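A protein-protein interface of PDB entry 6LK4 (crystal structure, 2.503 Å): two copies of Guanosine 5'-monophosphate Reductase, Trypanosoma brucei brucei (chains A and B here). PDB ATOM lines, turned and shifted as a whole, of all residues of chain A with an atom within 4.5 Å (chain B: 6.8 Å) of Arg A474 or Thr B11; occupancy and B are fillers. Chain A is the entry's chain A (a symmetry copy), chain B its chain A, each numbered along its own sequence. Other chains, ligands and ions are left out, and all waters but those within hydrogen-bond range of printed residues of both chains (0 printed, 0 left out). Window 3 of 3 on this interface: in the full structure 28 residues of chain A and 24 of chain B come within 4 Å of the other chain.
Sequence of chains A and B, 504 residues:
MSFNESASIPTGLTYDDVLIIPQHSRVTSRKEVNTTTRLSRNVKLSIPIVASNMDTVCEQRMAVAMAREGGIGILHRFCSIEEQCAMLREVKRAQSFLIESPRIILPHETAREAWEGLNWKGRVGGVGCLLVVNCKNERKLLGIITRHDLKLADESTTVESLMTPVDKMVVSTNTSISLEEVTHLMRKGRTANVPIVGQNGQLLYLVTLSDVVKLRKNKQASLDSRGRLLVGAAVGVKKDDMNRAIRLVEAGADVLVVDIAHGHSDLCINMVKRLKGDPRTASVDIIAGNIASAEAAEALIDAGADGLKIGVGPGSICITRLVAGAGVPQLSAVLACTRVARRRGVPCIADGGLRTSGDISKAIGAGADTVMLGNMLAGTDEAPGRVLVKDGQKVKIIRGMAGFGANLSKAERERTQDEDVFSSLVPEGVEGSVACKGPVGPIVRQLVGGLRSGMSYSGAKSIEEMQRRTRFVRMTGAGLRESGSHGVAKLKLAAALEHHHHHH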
ATOM      1  N   LEU A  13     -23.397  16.197 -24.843  1.00  0.00           N
ATOM      2  CA  LEU A  13     -22.367  16.544 -25.799  1.00  0.00           C
ATOM      3  C   LEU A  13     -22.072  15.358 -26.699  1.00  0.00           C
ATOM      4  O   LEU A  13     -21.981  14.211 -26.234  1.00  0.00           O
ATOM      5  CB  LEU A  13     -21.084  16.984 -25.090  1.00  0.00           C
ATOM      6  CG  LEU A  13     -21.213  18.084 -24.036  1.00  0.00           C
ATOM      7  CD1 LEU A  13     -19.898  18.275 -23.337  1.00  0.00           C
ATOM      8  CD2 LEU A  13     -21.628  19.384 -24.690  1.00  0.00           C
ATOM      9  N   ASP A  17     -18.804  18.482 -30.287  1.00  0.00           N
ATOM     10  CA  ASP A  17     -18.831  19.597 -29.346  1.00  0.00           C
ATOM     11  C   ASP A  17     -17.484  19.865 -28.684  1.00  0.00           C
ATOM     12  O   ASP A  17     -17.310  20.931 -28.081  1.00  0.00           O
ATOM     13  CB  ASP A  17     -19.855  19.344 -28.242  1.00  0.00           C
ATOM     14  CG  ASP A  17     -21.290  19.406 -28.747  1.00  0.00           C
ATOM     15  OD1 ASP A  17     -21.680  20.469 -29.271  1.00  0.00           O
ATOM     16  OD2 ASP A  17     -22.018  18.390 -28.625  1.00  0.00           O
ATOM     17  N   VAL A  18     -16.538  18.921 -28.734  1.00  0.00           N
ATOM     18  CA  VAL A  18     -15.340  19.040 -27.920  1.00  0.00           C
ATOM     19  C   VAL A  18     -14.080  18.823 -28.748  1.00  0.00           C
ATOM     20  O   VAL A  18     -14.102  18.248 -29.838  1.00  0.00           O
ATOM     21  CB  VAL A  18     -15.379  18.071 -26.735  1.00  0.00           C
ATOM     22  CG1 VAL A  18     -16.579  18.412 -25.871  1.00  0.00           C
ATOM     23  CG2 VAL A  18     -15.450  16.625 -27.219  1.00  0.00           C
ATOM     24  N   PHE A 472     -11.053  17.798 -22.154  1.00  0.00           N
ATOM     25  CA  PHE A 472     -11.804  18.334 -23.271  1.00  0.00           C
ATOM     26  C   PHE A 472     -12.015  19.828 -23.111  1.00  0.00           C
ATOM     27  O   PHE A 472     -12.044  20.353 -21.995  1.00  0.00           O
ATOM     28  CB  PHE A 472     -13.158  17.637 -23.379  1.00  0.00           C
ATOM     29  CG  PHE A 472     -13.056  16.217 -23.810  1.00  0.00           C
ATOM     30  CD1 PHE A 472     -12.606  15.904 -25.079  1.00  0.00           C
ATOM     31  CD2 PHE A 472     -13.388  15.190 -22.946  1.00  0.00           C
ATOM     32  CE1 PHE A 472     -12.508  14.590 -25.480  1.00  0.00           C
ATOM     33  CE2 PHE A 472     -13.286  13.877 -23.341  1.00  0.00           C
ATOM     34  CZ  PHE A 472     -12.850  13.576 -24.609  1.00  0.00           C
ATOM     35  N   VAL A 473     -12.192  20.501 -24.242  1.00  0.00           N
ATOM     36  CA  VAL A 473     -12.706  21.861 -24.274  1.00  0.00           C
ATOM     37  C   VAL A 473     -13.861  21.894 -25.265  1.00  0.00           C
ATOM     38  O   VAL A 473     -13.806  21.251 -26.320  1.00  0.00           O
ATOM     39  CB  VAL A 473     -11.603  22.884 -24.650  1.00  0.00           C
ATOM     40  CG1 VAL A 473     -11.075  22.632 -26.074  1.00  0.00           C
ATOM     41  CG2 VAL A 473     -12.110  24.297 -24.490  1.00  0.00           C
ATOM     42  N   ARG A 474     -14.904  22.646 -24.930  1.00  0.00           N
ATOM     43  CA  ARG A 474     -16.147  22.672 -25.686  1.00  0.00           C
ATOM     44  C   ARG A 474     -16.162  23.816 -26.689  1.00  0.00           C
ATOM     45  O   ARG A 474     -15.826  24.952 -26.349  1.00  0.00           O
ATOM     46  CB  ARG A 474     -17.299  22.846 -24.719  1.00  0.00           C
ATOM     47  CG  ARG A 474     -18.489  22.002 -24.940  1.00  0.00           C
ATOM     48  CD  ARG A 474     -19.516  22.419 -23.912  1.00  0.00           C
ATOM     49  NE  ARG A 474     -20.673  23.027 -24.546  1.00  0.00           N
ATOM     50  CZ  ARG A 474     -21.800  23.313 -23.907  1.00  0.00           C
ATOM     51  NH1 ARG A 474     -21.896  23.040 -22.612  1.00  0.00           N
ATOM     52  NH2 ARG A 474     -22.824  23.858 -24.564  1.00  0.00           N
ATOM     53  N   MET A 475     -16.571  23.526 -27.917  1.00  0.00           N
ATOM     54  CA  MET A 475     -16.716  24.559 -28.928  1.00  0.00           C
ATOM     55  C   MET A 475     -18.153  25.082 -28.962  1.00  0.00           C
ATOM     56  O   MET A 475     -19.023  24.663 -28.196  1.00  0.00           O
ATOM     57  CB  MET A 475     -16.347  24.045 -30.321  1.00  0.00           C
ATOM     58  CG  MET A 475     -14.886  23.782 -30.573  1.00  0.00           C
ATOM     59  SD  MET A 475     -14.737  22.249 -31.505  1.00  0.00           S
ATOM     60  CE  MET A 475     -14.801  22.809 -33.184  1.00  0.00           C
ATOM     61  N   THR A 476     -18.389  26.006 -29.897  1.00  0.00           N
ATOM     62  CA  THR A 476     -19.705  26.493 -30.297  1.00  0.00           C
ATOM     63  C   THR A 476     -19.757  26.561 -31.829  1.00  0.00           C
ATOM     64  O   THR A 476     -19.642  25.539 -32.521  1.00  0.00           O
ATOM     65  CB  THR A 476     -19.976  27.879 -29.699  1.00  0.00           C
ATOM     66  OG1 THR A 476     -19.094  28.803 -30.319  1.00  0.00           O
ATOM     67  CG2 THR A 476     -19.691  27.927 -28.211  1.00  0.00           C
ATOM     68  N   SER B   6     -20.304  16.061 -18.145  1.00  0.00           N
ATOM     69  CA  SER B   6     -20.335  16.930 -19.317  1.00  0.00           C
ATOM     70  C   SER B   6     -20.519  18.392 -18.925  1.00  0.00           C
ATOM     71  O   SER B   6     -19.924  19.280 -19.539  1.00  0.00           O
ATOM     72  CB  SER B   6     -21.438  16.478 -20.286  1.00  0.00           C
ATOM     73  OG  SER B   6     -21.501  15.055 -20.410  1.00  0.00           O
ATOM     74  N   ALA B   7     -21.322  18.666 -17.898  1.00  0.00           N
ATOM     75  CA  ALA B   7     -21.604  20.053 -17.532  1.00  0.00           C
ATOM     76  C   ALA B   7     -20.357  20.818 -17.114  1.00  0.00           C
ATOM     77  O   ALA B   7     -20.375  22.054 -17.113  1.00  0.00           O
ATOM     78  CB  ALA B   7     -22.641  20.104 -16.401  1.00  0.00           C
ATOM     79  N   ILE B   9     -17.199  20.614 -18.466  1.00  0.00           N
ATOM     80  CA  ILE B   9     -16.215  20.853 -19.513  1.00  0.00           C
ATOM     81  C   ILE B   9     -16.237  22.346 -19.839  1.00  0.00           C
ATOM     82  O   ILE B   9     -17.301  22.897 -20.140  1.00  0.00           O
ATOM     83  CB  ILE B   9     -16.519  19.958 -20.728  1.00  0.00           C
ATOM     84  CG1 ILE B   9     -16.277  18.499 -20.352  1.00  0.00           C
ATOM     85  CG2 ILE B   9     -15.696  20.334 -21.932  1.00  0.00           C
ATOM     86  CD1 ILE B   9     -16.716  17.515 -21.395  1.00  0.00           C
ATOM     87  N   PRO B  10     -15.117  23.052 -19.785  1.00  0.00           N
ATOM     88  CA  PRO B  10     -15.144  24.492 -20.080  1.00  0.00           C
ATOM     89  C   PRO B  10     -15.345  24.746 -21.566  1.00  0.00           C
ATOM     90  O   PRO B  10     -15.191  23.860 -22.411  1.00  0.00           O
ATOM     91  CB  PRO B  10     -13.771  24.972 -19.619  1.00  0.00           C
ATOM     92  CG  PRO B  10     -12.883  23.769 -19.816  1.00  0.00           C
ATOM     93  CD  PRO B  10     -13.757  22.570 -19.474  1.00  0.00           C
ATOM     94  N   THR B  11     -15.671  25.997 -21.886  1.00  0.00           N
ATOM     95  CA  THR B  11     -16.003  26.389 -23.249  1.00  0.00           C
ATOM     96  C   THR B  11     -14.924  27.304 -23.808  1.00  0.00           C
ATOM     97  O   THR B  11     -14.480  28.232 -23.131  1.00  0.00           O
ATOM     98  CB  THR B  11     -17.362  27.081 -23.290  1.00  0.00           C
ATOM     99  OG1 THR B  11     -18.370  26.158 -22.858  1.00  0.00           O
ATOM    100  CG2 THR B  11     -17.670  27.570 -24.692  1.00  0.00           C
ATOM    101  N   GLY B  12     -14.495  27.028 -25.033  1.00  0.00           N
ATOM    102  CA  GLY B  12     -13.473  27.809 -25.698  1.00  0.00           C
ATOM    103  C   GLY B  12     -14.062  28.614 -26.840  1.00  0.00           C
ATOM    104  O   GLY B  12     -14.995  28.171 -27.523  1.00  0.00           O
ATOM    105  N   LEU B  13     -13.505  29.802 -27.047  1.00  0.00           N
ATOM    106  CA  LEU B  13     -14.008  30.742 -28.026  1.00  0.00           C
ATOM    107  C   LEU B  13     -12.992  30.928 -29.138  1.00  0.00           C
ATOM    108  O   LEU B  13     -11.782  31.042 -28.885  1.00  0.00           O
ATOM    109  CB  LEU B  13     -14.319  32.094 -27.382  1.00  0.00           C
ATOM    110  CG  LEU B  13     -15.225  32.087 -26.150  1.00  0.00           C
ATOM    111  CD1 LEU B  13     -15.292  33.466 -25.560  1.00  0.00           C
ATOM    112  CD2 LEU B  13     -16.617  31.635 -26.531  1.00  0.00           C
ATOM    113  N   PRO B 329      -9.940  26.433 -29.288  1.00  0.00           N
ATOM    114  CA  PRO B 329     -10.443  27.623 -29.972  1.00  0.00           C
ATOM    115  C   PRO B 329      -9.506  28.794 -29.727  1.00  0.00           C
ATOM    116  O   PRO B 329      -9.090  29.055 -28.597  1.00  0.00           O
ATOM    117  CB  PRO B 329     -11.825  27.821 -29.353  1.00  0.00           C
ATOM    118  CG  PRO B 329     -12.249  26.421 -29.006  1.00  0.00           C
ATOM    119  CD  PRO B 329     -10.999  25.746 -28.528  1.00  0.00           C
ATOM    120  N   SER B 332      -9.630  31.877 -26.919  1.00  0.00           N
ATOM    121  CA  SER B 332      -9.270  31.374 -25.596  1.00  0.00           C
ATOM    122  C   SER B 332      -7.784  31.096 -25.496  1.00  0.00           C
ATOM    123  O   SER B 332      -7.145  31.445 -24.489  1.00  0.00           O
ATOM    124  CB  SER B 332     -10.057  30.101 -25.282  1.00  0.00           C
ATOM    125  OG  SER B 332     -11.440  30.326 -25.433  1.00  0.00           O
ATOM    126  N   ARG B 474     -19.864  38.362 -26.869  1.00  0.00           N
ATOM    127  CA  ARG B 474     -20.019  37.053 -27.485  1.00  0.00           C
ATOM    128  C   ARG B 474     -21.317  36.962 -28.274  1.00  0.00           C
ATOM    129  O   ARG B 474     -22.378  37.349 -27.781  1.00  0.00           O
ATOM    130  CB  ARG B 474     -20.028  36.001 -26.395  1.00  0.00           C
ATOM    131  CG  ARG B 474     -19.235  34.782 -26.639  1.00  0.00           C
ATOM    132  CD  ARG B 474     -19.473  33.866 -25.460  1.00  0.00           C
ATOM    133  NE  ARG B 474     -20.182  32.663 -25.866  1.00  0.00           N
ATOM    134  CZ  ARG B 474     -20.357  31.609 -25.081  1.00  0.00           C
ATOM    135  NH1 ARG B 474     -19.867  31.632 -23.848  1.00  0.00           N
ATOM    136  NH2 ARG B 474     -21.006  30.536 -25.533  1.00  0.00           N
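N of Gly B12 sits at hydrogen-bond distance from O of Arg A474 (2.8 Å).
The backbone NH (N) of Arg A474 lies within hydrogen-bond range of the backbone carbonyl oxygen (O) of Pro B10 (2.8 Å).
Leu A13 touches Ser B6.
CD1 of Leu A13 touches CD1 of Ile B9, at 3.8 Å.
CG2 of Ile B9 touches O of Phe A472, at 3.7 Å.
Phe A472 touches Pro B10 (O to CD, 3.8 Å).
Val A473 touches Pro B10.
Gly B12 touches Val A473.
Pro B329 touches Val A473 (CD to CG1, 3.97 Å).
Arg A474 touches Ile B9 (N to CG2, 3.9 Å).
Thr B11 touches Arg A474 (CA to O, 3.4 Å).
Arg B474 touches Thr A476 (NH2 to CG2, 3.96 Å).
Of chain B, only Ile B9 (3.9 Å), Pro B10 (2.8 Å), Thr B11 (3.4 Å) and Gly B12 (2.8 Å) come within 4 Å of Arg A474.
Printed residues of chain B within 4 Å of Thr A476: Arg B474.
Printed residues of chain A within 4 Å of Ser B6: Leu A13 (3.9 Å).
Ala B7 touches none of the printed residues of chain A.
Of the 8 printed residues of chain A, 5 touch a printed residue of chain B.
Hydrophobic or aromatic side chains of chain A that line the printed part of chain B: Leu A13, Phe A472 and Val A473.
Along chain A the printed residues that touch a printed residue of chain B span positions 13 to 476.
Among the printed residues, no Asp or Glu carboxylate lies within 4 Å of a Lys or Arg side-chain nitrogen of the other chain.
Positions printed for both chains: 13 and 474.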
